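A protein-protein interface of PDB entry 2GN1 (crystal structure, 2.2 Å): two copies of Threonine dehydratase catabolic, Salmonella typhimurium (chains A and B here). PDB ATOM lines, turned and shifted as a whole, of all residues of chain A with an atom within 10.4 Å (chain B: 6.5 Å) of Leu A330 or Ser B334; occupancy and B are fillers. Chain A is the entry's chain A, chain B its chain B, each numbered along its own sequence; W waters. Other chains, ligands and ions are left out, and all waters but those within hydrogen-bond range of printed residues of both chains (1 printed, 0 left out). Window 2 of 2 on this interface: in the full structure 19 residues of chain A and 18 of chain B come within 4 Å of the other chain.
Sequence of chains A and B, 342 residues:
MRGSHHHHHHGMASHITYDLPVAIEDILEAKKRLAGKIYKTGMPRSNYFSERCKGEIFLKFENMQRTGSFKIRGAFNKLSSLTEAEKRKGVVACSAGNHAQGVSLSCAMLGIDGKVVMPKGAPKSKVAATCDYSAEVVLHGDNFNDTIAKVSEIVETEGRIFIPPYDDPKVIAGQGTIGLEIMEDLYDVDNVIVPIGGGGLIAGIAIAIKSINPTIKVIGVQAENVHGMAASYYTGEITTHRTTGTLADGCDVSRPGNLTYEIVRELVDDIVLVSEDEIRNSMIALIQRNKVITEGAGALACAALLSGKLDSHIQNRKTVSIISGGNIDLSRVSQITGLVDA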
ATOM      1  N   PRO A 123      -8.880  14.415  -4.405  1.00  0.00           N
ATOM      2  CA  PRO A 123      -8.496  14.411  -5.817  1.00  0.00           C
ATOM      3  C   PRO A 123      -6.986  14.589  -5.984  1.00  0.00           C
ATOM      4  O   PRO A 123      -6.418  15.564  -5.486  1.00  0.00           O
ATOM      5  CB  PRO A 123      -9.257  15.606  -6.395  1.00  0.00           C
ATOM      6  CG  PRO A 123     -10.440  15.775  -5.488  1.00  0.00           C
ATOM      7  CD  PRO A 123      -9.986  15.350  -4.127  1.00  0.00           C
ATOM      8  N   SER A 125      -5.119  15.672  -8.164  1.00  0.00           N
ATOM      9  CA  SER A 125      -4.692  16.966  -8.701  1.00  0.00           C
ATOM     10  C   SER A 125      -4.472  17.996  -7.591  1.00  0.00           C
ATOM     11  O   SER A 125      -3.533  18.792  -7.659  1.00  0.00           O
ATOM     12  CB  SER A 125      -5.706  17.501  -9.727  1.00  0.00           C
ATOM     13  OG  SER A 125      -6.996  17.675  -9.166  1.00  0.00           O
ATOM     14  N   LYS A 126      -5.340  17.971  -6.580  1.00  0.00           N
ATOM     15  CA  LYS A 126      -5.259  18.899  -5.446  1.00  0.00           C
ATOM     16  C   LYS A 126      -4.097  18.515  -4.522  1.00  0.00           C
ATOM     17  O   LYS A 126      -3.372  19.376  -4.019  1.00  0.00           O
ATOM     18  CB  LYS A 126      -6.582  18.914  -4.665  1.00  0.00           C
ATOM     19  CG  LYS A 126      -7.796  19.363  -5.480  1.00  0.00           C
ATOM     20  CD  LYS A 126      -9.100  19.178  -4.713  1.00  0.00           C
ATOM     21  CE  LYS A 126     -10.322  19.661  -5.509  1.00  0.00           C
ATOM     22  NZ  LYS A 126     -10.515  21.153  -5.462  1.00  0.00           N
ATOM     23  N   MET A 283     -23.041  26.428 -13.574  1.00  0.00           N
ATOM     24  CA  MET A 283     -21.740  25.963 -14.075  1.00  0.00           C
ATOM     25  C   MET A 283     -21.748  25.883 -15.602  1.00  0.00           C
ATOM     26  O   MET A 283     -20.834  26.366 -16.258  1.00  0.00           O
ATOM     27  CB  MET A 283     -21.373  24.602 -13.475  1.00  0.00           C
ATOM     28  CG  MET A 283     -21.136  24.626 -11.957  1.00  0.00           C
ATOM     29  SD  MET A 283     -20.847  22.986 -11.244  1.00  0.00           S
ATOM     30  CE  MET A 283     -19.260  22.574 -11.960  1.00  0.00           C
ATOM     31  N   ILE A 287     -19.327  28.212 -18.104  1.00  0.00           N
ATOM     32  CA  ILE A 287     -18.342  27.602 -19.003  1.00  0.00           C
ATOM     33  C   ILE A 287     -18.728  27.741 -20.478  1.00  0.00           C
ATOM     34  O   ILE A 287     -17.907  28.169 -21.288  1.00  0.00           O
ATOM     35  CB  ILE A 287     -18.054  26.120 -18.628  1.00  0.00           C
ATOM     36  CG1 ILE A 287     -17.648  26.013 -17.147  1.00  0.00           C
ATOM     37  CG2 ILE A 287     -16.926  25.558 -19.501  1.00  0.00           C
ATOM     38  CD1 ILE A 287     -18.066  24.709 -16.468  1.00  0.00           C
ATOM     39  N   LYS A 291     -17.315  31.200 -21.004  1.00  0.00           N
ATOM     40  CA  LYS A 291     -15.958  30.702 -21.266  1.00  0.00           C
ATOM     41  C   LYS A 291     -15.018  30.779 -20.066  1.00  0.00           C
ATOM     42  O   LYS A 291     -13.816  30.974 -20.218  1.00  0.00           O
ATOM     43  CB  LYS A 291     -15.355  31.417 -22.484  1.00  0.00           C
ATOM     44  CG  LYS A 291     -16.227  31.369 -23.723  1.00  0.00           C
ATOM     45  CD  LYS A 291     -16.518  29.935 -24.179  1.00  0.00           C
ATOM     46  CE  LYS A 291     -17.457  29.886 -25.366  1.00  0.00           C
ATOM     47  NZ  LYS A 291     -17.554  28.504 -25.948  1.00  0.00           N
ATOM     48  N   VAL A 292     -15.567  30.601 -18.868  1.00  0.00           N
ATOM     49  CA  VAL A 292     -14.746  30.562 -17.664  1.00  0.00           C
ATOM     50  C   VAL A 292     -14.945  29.246 -16.923  1.00  0.00           C
ATOM     51  O   VAL A 292     -16.071  28.741 -16.825  1.00  0.00           O
ATOM     52  CB  VAL A 292     -15.017  31.765 -16.721  1.00  0.00           C
ATOM     53  CG1 VAL A 292     -14.310  33.017 -17.236  1.00  0.00           C
ATOM     54  CG2 VAL A 292     -16.511  32.033 -16.574  1.00  0.00           C
ATOM     55  N   ILE A 293     -13.842  28.687 -16.433  1.00  0.00           N
ATOM     56  CA  ILE A 293     -13.881  27.464 -15.634  1.00  0.00           C
ATOM     57  C   ILE A 293     -14.141  27.826 -14.171  1.00  0.00           C
ATOM     58  O   ILE A 293     -13.412  28.622 -13.559  1.00  0.00           O
ATOM     59  CB  ILE A 293     -12.589  26.642 -15.769  1.00  0.00           C
ATOM     60  CG1 ILE A 293     -12.416  26.199 -17.224  1.00  0.00           C
ATOM     61  CG2 ILE A 293     -12.615  25.413 -14.859  1.00  0.00           C
ATOM     62  CD1 ILE A 293     -11.081  25.585 -17.510  1.00  0.00           C
ATOM     63  N   THR A 294     -15.196  27.228 -13.633  1.00  0.00           N
ATOM     64  CA  THR A 294     -15.603  27.422 -12.255  1.00  0.00           C
ATOM     65  C   THR A 294     -15.863  26.056 -11.650  1.00  0.00           C
ATOM     66  O   THR A 294     -16.350  25.151 -12.330  1.00  0.00           O
ATOM     67  CB  THR A 294     -16.898  28.295 -12.151  1.00  0.00           C
ATOM     68  OG1 THR A 294     -17.329  28.367 -10.782  1.00  0.00           O
ATOM     69  CG2 THR A 294     -18.028  27.721 -12.991  1.00  0.00           C
ATOM     70  N   GLU A 295     -15.503  25.905 -10.386  1.00  0.00           N
ATOM     71  CA  GLU A 295     -15.913  24.744  -9.595  1.00  0.00           C
ATOM     72  C   GLU A 295     -17.304  25.029  -9.062  1.00  0.00           C
ATOM     73  O   GLU A 295     -17.805  26.144  -9.204  1.00  0.00           O
ATOM     74  CB  GLU A 295     -14.923  24.461  -8.456  1.00  0.00           C
ATOM     75  CG  GLU A 295     -14.880  25.507  -7.362  1.00  0.00           C
ATOM     76  CD  GLU A 295     -13.798  25.216  -6.363  1.00  0.00           C
ATOM     77  OE1 GLU A 295     -12.667  25.684  -6.570  1.00  0.00           O
ATOM     78  OE2 GLU A 295     -14.075  24.491  -5.388  1.00  0.00           O
ATOM     79  N   GLY A 326     -11.997  28.071  -9.147  1.00  0.00           N
ATOM     80  CA  GLY A 326     -11.980  27.337 -10.393  1.00  0.00           C
ATOM     81  C   GLY A 326     -11.245  26.025 -10.303  1.00  0.00           C
ATOM     82  O   GLY A 326     -10.763  25.526 -11.317  1.00  0.00           O
ATOM     83  N   ASN A 327     -11.166  25.462  -9.095  1.00  0.00           N
ATOM     84  CA  ASN A 327     -10.401  24.241  -8.865  1.00  0.00           C
ATOM     85  C   ASN A 327     -11.282  22.999  -8.994  1.00  0.00           C
ATOM     86  O   ASN A 327     -11.832  22.464  -8.025  1.00  0.00           O
ATOM     87  CB  ASN A 327      -9.654  24.296  -7.535  1.00  0.00           C
ATOM     88  CG  ASN A 327      -8.500  25.283  -7.565  1.00  0.00           C
ATOM     89  OD1 ASN A 327      -7.885  25.486  -8.604  1.00  0.00           O
ATOM     90  ND2 ASN A 327      -8.217  25.916  -6.434  1.00  0.00           N
ATOM     91  N   ILE A 328     -11.401  22.566 -10.235  1.00  0.00           N
ATOM     92  CA  ILE A 328     -12.148  21.384 -10.589  1.00  0.00           C
ATOM     93  C   ILE A 328     -11.429  20.787 -11.782  1.00  0.00           C
ATOM     94  O   ILE A 328     -10.963  21.516 -12.663  1.00  0.00           O
ATOM     95  CB  ILE A 328     -13.618  21.737 -10.901  1.00  0.00           C
ATOM     96  CG1 ILE A 328     -14.420  20.486 -11.276  1.00  0.00           C
ATOM     97  CG2 ILE A 328     -13.697  22.805 -11.990  1.00  0.00           C
ATOM     98  CD1 ILE A 328     -15.901  20.778 -11.573  1.00  0.00           C
ATOM     99  N   ASP A 329     -11.302  19.465 -11.787  1.00  0.00           N
ATOM    100  CA  ASP A 329     -10.701  18.762 -12.910  1.00  0.00           C
ATOM    101  C   ASP A 329     -11.545  18.968 -14.159  1.00  0.00           C
ATOM    102  O   ASP A 329     -12.763  18.844 -14.119  1.00  0.00           O
ATOM    103  CB  ASP A 329     -10.561  17.265 -12.607  1.00  0.00           C
ATOM    104  CG  ASP A 329      -9.425  16.963 -11.632  1.00  0.00           C
ATOM    105  OD1 ASP A 329      -8.423  17.714 -11.615  1.00  0.00           O
ATOM    106  OD2 ASP A 329      -9.528  15.961 -10.892  1.00  0.00           O
ATOM    107  N   LEU A 330     -10.873  19.280 -15.262  1.00  0.00           N
ATOM    108  CA  LEU A 330     -11.509  19.490 -16.553  1.00  0.00           C
ATOM    109  C   LEU A 330     -12.397  18.304 -16.956  1.00  0.00           C
ATOM    110  O   LEU A 330     -13.418  18.491 -17.610  1.00  0.00           O
ATOM    111  CB  LEU A 330     -10.430  19.725 -17.615  1.00  0.00           C
ATOM    112  CG  LEU A 330     -10.888  20.024 -19.039  1.00  0.00           C
ATOM    113  CD1 LEU A 330     -11.595  21.367 -19.116  1.00  0.00           C
ATOM    114  CD2 LEU A 330      -9.706  19.983 -19.985  1.00  0.00           C
ATOM    115  N   SER A 331     -11.996  17.095 -16.557  1.00  0.00           N
ATOM    116  CA  SER A 331     -12.815  15.891 -16.736  1.00  0.00           C
ATOM    117  C   SER A 331     -14.182  15.974 -16.041  1.00  0.00           C
ATOM    118  O   SER A 331     -15.184  15.491 -16.575  1.00  0.00           O
ATOM    119  CB  SER A 331     -12.065  14.661 -16.207  1.00  0.00           C
ATOM    120  OG  SER A 331     -11.873  14.764 -14.804  1.00  0.00           O
ATOM    121  N   ARG A 332     -14.210  16.567 -14.847  1.00  0.00           N
ATOM    122  CA  ARG A 332     -15.441  16.673 -14.070  1.00  0.00           C
ATOM    123  C   ARG A 332     -16.338  17.773 -14.634  1.00  0.00           C
ATOM    124  O   ARG A 332     -17.562  17.634 -14.659  1.00  0.00           O
ATOM    125  CB  ARG A 332     -15.139  16.932 -12.588  1.00  0.00           C
ATOM    126  CG  ARG A 332     -16.285  16.529 -11.656  1.00  0.00           C
ATOM    127  CD  ARG A 332     -15.947  16.768 -10.185  1.00  0.00           C
ATOM    128  NE  ARG A 332     -17.145  16.998  -9.372  1.00  0.00           N
ATOM    129  CZ  ARG A 332     -17.149  17.536  -8.147  1.00  0.00           C
ATOM    130  NH1 ARG A 332     -16.013  17.907  -7.559  1.00  0.00           N
ATOM    131  NH2 ARG A 332     -18.301  17.709  -7.506  1.00  0.00           N
ATOM    132  N   VAL A 333     -15.714  18.863 -15.072  1.00  0.00           N
ATOM    133  CA  VAL A 333     -16.401  19.949 -15.773  1.00  0.00           C
ATOM    134  C   VAL A 333     -17.133  19.403 -17.002  1.00  0.00           C
ATOM    135  O   VAL A 333     -18.253  19.814 -17.289  1.00  0.00           O
ATOM    136  CB  VAL A 333     -15.393  21.058 -16.206  1.00  0.00           C
ATOM    137  CG1 VAL A 333     -15.997  21.999 -17.247  1.00  0.00           C
ATOM    138  CG2 VAL A 333     -14.930  21.826 -15.013  1.00  0.00           C
ATOM    139  N   SER A 334     -16.493  18.471 -17.704  1.00  0.00           N
ATOM    140  CA  SER A 334     -17.069  17.845 -18.897  1.00  0.00           C
ATOM    141  C   SER A 334     -18.295  16.985 -18.587  1.00  0.00           C
ATOM    142  O   SER A 334     -19.302  17.061 -19.295  1.00  0.00           O
ATOM    143  CB  SER A 334     -16.016  16.988 -19.604  1.00  0.00           C
ATOM    144  OG  SER A 334     -14.866  17.750 -19.919  1.00  0.00           O
ATOM    145  N   GLN A 335     -18.211  16.166 -17.539  1.00  0.00           N
ATOM    146  CA  GLN A 335     -19.332  15.287 -17.179  1.00  0.00           C
ATOM    147  C   GLN A 335     -20.455  16.043 -16.464  1.00  0.00           C
ATOM    148  O   GLN A 335     -21.620  15.677 -16.585  1.00  0.00           O
ATOM    149  CB  GLN A 335     -18.873  14.068 -16.361  1.00  0.00           C
ATOM    150  CG  GLN A 335     -18.129  14.380 -15.082  1.00  0.00           C
ATOM    151  CD  GLN A 335     -17.857  13.148 -14.227  1.00  0.00           C
ATOM    152  OE1 GLN A 335     -17.967  12.013 -14.690  1.00  0.00           O
ATOM    153  NE2 GLN A 335     -17.495  13.374 -12.967  1.00  0.00           N
ATOM    154  N   ILE A 336     -20.114  17.101 -15.732  1.00  0.00           N
ATOM    155  CA  ILE A 336     -21.140  17.962 -15.130  1.00  0.00           C
ATOM    156  C   ILE A 336     -21.839  18.804 -16.205  1.00  0.00           C
ATOM    157  O   ILE A 336     -23.063  18.955 -16.183  1.00  0.00           O
ATOM    158  CB  ILE A 336     -20.563  18.881 -14.035  1.00  0.00           C
ATOM    159  CG1 ILE A 336     -20.162  18.051 -12.813  1.00  0.00           C
ATOM    160  CG2 ILE A 336     -21.596  19.933 -13.623  1.00  0.00           C
ATOM    161  CD1 ILE A 336     -19.344  18.820 -11.784  1.00  0.00           C
ATOM    162  N   THR A 337     -21.057  19.333 -17.142  1.00  0.00           N
ATOM    163  CA  THR A 337     -21.581  20.165 -18.224  1.00  0.00           C
ATOM    164  C   THR A 337     -22.068  19.297 -19.379  1.00  0.00           C
ATOM    165  O   THR A 337     -22.465  18.148 -19.174  1.00  0.00           O
ATOM    166  CB  THR A 337     -20.503  21.159 -18.693  1.00  0.00           C
ATOM    167  N   GLY A 338     -22.064  19.851 -20.590  1.00  0.00           N
ATOM    168  CA  GLY A 338     -22.361  19.077 -21.795  1.00  0.00           C
ATOM    169  C   GLY A 338     -21.199  18.172 -22.168  1.00  0.00           C
ATOM    170  O   GLY A 338     -20.039  18.469 -21.868  1.00  0.00           O
ATOM    171  N   ILE B 287      -6.501  27.694 -20.023  1.00  0.00           N
ATOM    172  CA  ILE B 287      -7.576  26.956 -19.351  1.00  0.00           C
ATOM    173  C   ILE B 287      -7.164  26.483 -17.952  1.00  0.00           C
ATOM    174  O   ILE B 287      -7.941  26.549 -17.007  1.00  0.00           O
ATOM    175  CB  ILE B 287      -8.080  25.753 -20.197  1.00  0.00           C
ATOM    176  CG1 ILE B 287      -7.145  24.541 -20.097  1.00  0.00           C
ATOM    177  N   ILE B 293     -11.764  29.442 -21.177  1.00  0.00           N
ATOM    178  CA  ILE B 293     -11.891  28.551 -22.323  1.00  0.00           C
ATOM    179  C   ILE B 293     -11.489  29.296 -23.590  1.00  0.00           C
ATOM    180  O   ILE B 293     -12.133  30.281 -23.987  1.00  0.00           O
ATOM    181  CB  ILE B 293     -13.323  27.986 -22.466  1.00  0.00           C
ATOM    182  CG1 ILE B 293     -13.728  27.183 -21.217  1.00  0.00           C
ATOM    183  CG2 ILE B 293     -13.445  27.120 -23.728  1.00  0.00           C
ATOM    184  CD1 ILE B 293     -12.914  25.910 -20.988  1.00  0.00           C
ATOM    185  N   ASP B 329     -15.234  22.706 -28.660  1.00  0.00           N
ATOM    186  CA  ASP B 329     -15.876  21.699 -27.835  1.00  0.00           C
ATOM    187  C   ASP B 329     -14.939  21.318 -26.701  1.00  0.00           C
ATOM    188  O   ASP B 329     -13.726  21.223 -26.882  1.00  0.00           O
ATOM    189  CB  ASP B 329     -16.238  20.462 -28.663  1.00  0.00           C
ATOM    190  CG  ASP B 329     -17.309  20.745 -29.695  1.00  0.00           C
ATOM    191  OD1 ASP B 329     -18.249  21.514 -29.398  1.00  0.00           O
ATOM    192  OD2 ASP B 329     -17.211  20.196 -30.812  1.00  0.00           O
ATOM    193  N   LEU B 330     -15.518  21.105 -25.531  1.00  0.00           N
ATOM    194  CA  LEU B 330     -14.759  20.747 -24.335  1.00  0.00           C
ATOM    195  C   LEU B 330     -13.944  19.458 -24.535  1.00  0.00           C
ATOM    196  O   LEU B 330     -12.846  19.329 -23.994  1.00  0.00           O
ATOM    197  CB  LEU B 330     -15.716  20.609 -23.142  1.00  0.00           C
ATOM    198  CG  LEU B 330     -15.341  21.285 -21.820  1.00  0.00           C
ATOM    199  CD1 LEU B 330     -14.713  22.664 -21.999  1.00  0.00           C
ATOM    200  CD2 LEU B 330     -16.593  21.372 -20.955  1.00  0.00           C
ATOM    201  N   SER B 331     -14.482  18.519 -25.313  1.00  0.00           N
ATOM    202  CA  SER B 331     -13.775  17.280 -25.633  1.00  0.00           C
ATOM    203  C   SER B 331     -12.518  17.557 -26.453  1.00  0.00           C
ATOM    204  O   SER B 331     -11.507  16.881 -26.284  1.00  0.00           O
ATOM    205  CB  SER B 331     -14.683  16.307 -26.397  1.00  0.00           C
ATOM    206  OG  SER B 331     -14.934  16.767 -27.711  1.00  0.00           O
ATOM    207  N   ARG B 332     -12.592  18.557 -27.331  1.00  0.00           N
ATOM    208  CA  ARG B 332     -11.448  18.951 -28.139  1.00  0.00           C
ATOM    209  C   ARG B 332     -10.410  19.675 -27.282  1.00  0.00           C
ATOM    210  O   ARG B 332      -9.206  19.485 -27.464  1.00  0.00           O
ATOM    211  CB  ARG B 332     -11.885  19.820 -29.320  1.00  0.00           C
ATOM    212  CG  ARG B 332     -10.839  19.895 -30.406  1.00  0.00           C
ATOM    213  CD  ARG B 332     -11.282  20.739 -31.579  1.00  0.00           C
ATOM    214  NE  ARG B 332     -10.127  21.180 -32.357  1.00  0.00           N
ATOM    215  CZ  ARG B 332     -10.165  22.076 -33.339  1.00  0.00           C
ATOM    216  NH1 ARG B 332     -11.316  22.649 -33.692  1.00  0.00           N
ATOM    217  NH2 ARG B 332      -9.040  22.400 -33.971  1.00  0.00           N
ATOM    218  N   VAL B 333     -10.879  20.484 -26.336  1.00  0.00           N
ATOM    219  CA  VAL B 333      -9.997  21.091 -25.328  1.00  0.00           C
ATOM    220  C   VAL B 333      -9.263  20.000 -24.537  1.00  0.00           C
ATOM    221  O   VAL B 333      -8.058  20.103 -24.321  1.00  0.00           O
ATOM    222  CB  VAL B 333     -10.778  22.007 -24.334  1.00  0.00           C
ATOM    223  CG1 VAL B 333      -9.885  22.446 -23.166  1.00  0.00           C
ATOM    224  CG2 VAL B 333     -11.326  23.214 -25.056  1.00  0.00           C
ATOM    225  N   SER B 334      -9.997  18.958 -24.135  1.00  0.00           N
ATOM    226  CA  SER B 334      -9.435  17.852 -23.348  1.00  0.00           C
ATOM    227  C   SER B 334      -8.409  17.052 -24.142  1.00  0.00           C
ATOM    228  O   SER B 334      -7.401  16.607 -23.599  1.00  0.00           O
ATOM    229  CB  SER B 334     -10.547  16.910 -22.866  1.00  0.00           C
ATOM    230  OG  SER B 334     -11.536  17.611 -22.133  1.00  0.00           O
ATOM    231  N   GLN B 335      -8.694  16.865 -25.426  1.00  0.00           N
ATOM    232  CA  GLN B 335      -7.790  16.201 -26.357  1.00  0.00           C
ATOM    233  C   GLN B 335      -6.458  16.948 -26.454  1.00  0.00           C
ATOM    234  O   GLN B 335      -5.384  16.354 -26.321  1.00  0.00           O
ATOM    235  CB  GLN B 335      -8.449  16.138 -27.736  1.00  0.00           C
ATOM    236  CG  GLN B 335      -7.874  15.106 -28.673  1.00  0.00           C
ATOM    237  CD  GLN B 335      -8.634  15.041 -29.993  1.00  0.00           C
ATOM    238  OE1 GLN B 335      -8.915  16.072 -30.613  1.00  0.00           O
ATOM    239  NE2 GLN B 335      -8.964  13.829 -30.431  1.00  0.00           N
ATOM    240  N   ILE B 336      -6.554  18.259 -26.669  1.00  0.00           N
ATOM    241  CA  ILE B 336      -5.399  19.133 -26.849  1.00  0.00           C
ATOM    242  C   ILE B 336      -4.699  19.399 -25.513  1.00  0.00           C
ATOM    243  O   ILE B 336      -3.478  19.278 -25.419  1.00  0.00           O
ATOM    244  CB  ILE B 336      -5.833  20.477 -27.509  1.00  0.00           C
ATOM    245  CG1 ILE B 336      -6.362  20.224 -28.931  1.00  0.00           C
ATOM    246  CG2 ILE B 336      -4.681  21.474 -27.539  1.00  0.00           C
ATOM    247  CD1 ILE B 336      -7.209  21.363 -29.502  1.00  0.00           C
ATOM    248  N   THR B 337      -5.473  19.743 -24.485  1.00  0.00           N
ATOM    249  CA  THR B 337      -4.929  20.034 -23.153  1.00  0.00           C
ATOM    250  C   THR B 337      -4.860  18.803 -22.238  1.00  0.00           C
ATOM    251  O   THR B 337      -4.822  18.949 -21.008  1.00  0.00           O
ATOM    252  CB  THR B 337      -5.751  21.146 -22.476  1.00  0.00           C
ATOM    253  N   GLY B 338      -4.822  17.603 -22.825  1.00  0.00           N
ATOM    254  CA  GLY B 338      -4.840  16.358 -22.054  1.00  0.00           C
ATOM    255  C   GLY B 338      -3.457  15.874 -21.672  1.00  0.00           C
ATOM    256  O   GLY B 338      -3.314  14.968 -20.850  1.00  0.00           O
HETATM  257  O   HOH W   1     -10.303  16.152 -19.280  1.00  0.00           O
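Among the printed residues, merely in contact across the chains: Ile A293 with Ile B287 (3.3 Å), Leu A330 with Ser B334 (3.7 Å), Val A333 with Leu B330 (3.8 Å), Ile A293 with Ile B293 (3.8 Å) and Ile A287 with Ile B293 (3.98 Å).
Of chain B, only Ser B334 comes within 4 Å of Leu A330.
Of chain A, only Val A333 comes within 4 Å of Leu B330.
No residue of chain A comes within 4 Å of Thr B337.
Gly B338 touches none of the printed residues of chain A.
Printed residues of chain B within 4 Å of Ile A293: Ile B287 and Ile B293.
Of the printed residues of chain A, Ile B287 touches Ile A293 (3.3 Å).
Of the printed residues of chain B, Ile A287 touches Ile B293 (3.98 Å).
Of the printed residues of chain B, Val A333 touches Leu B330.
Printed residues of chain B within 4 Å of Lys A291: Ile B293.
The nearest printed residue of chain A that does not touch Ser B334 is Ser A334 (4.001 Å).
The nearest printed residue of chain B that does not touch Lys A291 is Asp B329 (6.8 Å).
The side-chain hydroxyl (OG) of Ser A334 sits at hydrogen-bond distance from the backbone carbonyl oxygen (O) of Leu A330, at 2.8 Å.
The side-chain hydroxyl of Ser B334 is in hydrogen-bond range of the backbone carbonyl oxygen of Leu B330 (2.9 Å).
Printed residues of chain A that touch a printed residue of chain B: Ile A287, Lys A291, Ile A293, Leu A330 and Val A333.
Hydrophobic or aromatic side chains of chain A that line the printed part of chain B: Ile A287, Ile A293, Leu A330 and Val A333.
Hydrophobic or aromatic side chains of chain B that line the printed part of chain A: Ile B293 and Leu B330.
Along chain B the printed residues that touch a printed residue of chain A span positions 287 to 334.
Among the printed residues, no Asp or Glu carboxylate lies within 4 Å of a Lys or Arg side-chain nitrogen of the other chain.
Ile A287 touches Ile B293, and with the chains exchanged Ile A293 touches Ile B287.
Ile B293 touches its own counterpart, Ile A293.
Leu A330 touches Ser B334, but with the chains exchanged Ser A334 does not touch Leu B330 (4.04 Å).
Val A333 touches Leu B330, but with the chains exchanged Leu A330 does not touch Val B333 (4.03 Å).
Positions printed for both chains: 287, 293, 329, 330, 331, 332, 333, 334, 335, 336, 337 and 338.
Water W1 lies within hydrogen-bond range of the backbone NH (N) of Ser A331 (3.3 Å) and the side-chain hydroxyl (OG) of Ser B334 (3.4 Å).
O of Lys A291 is in hydrogen-bond range of N of Ile B293, at 2.7 Å.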
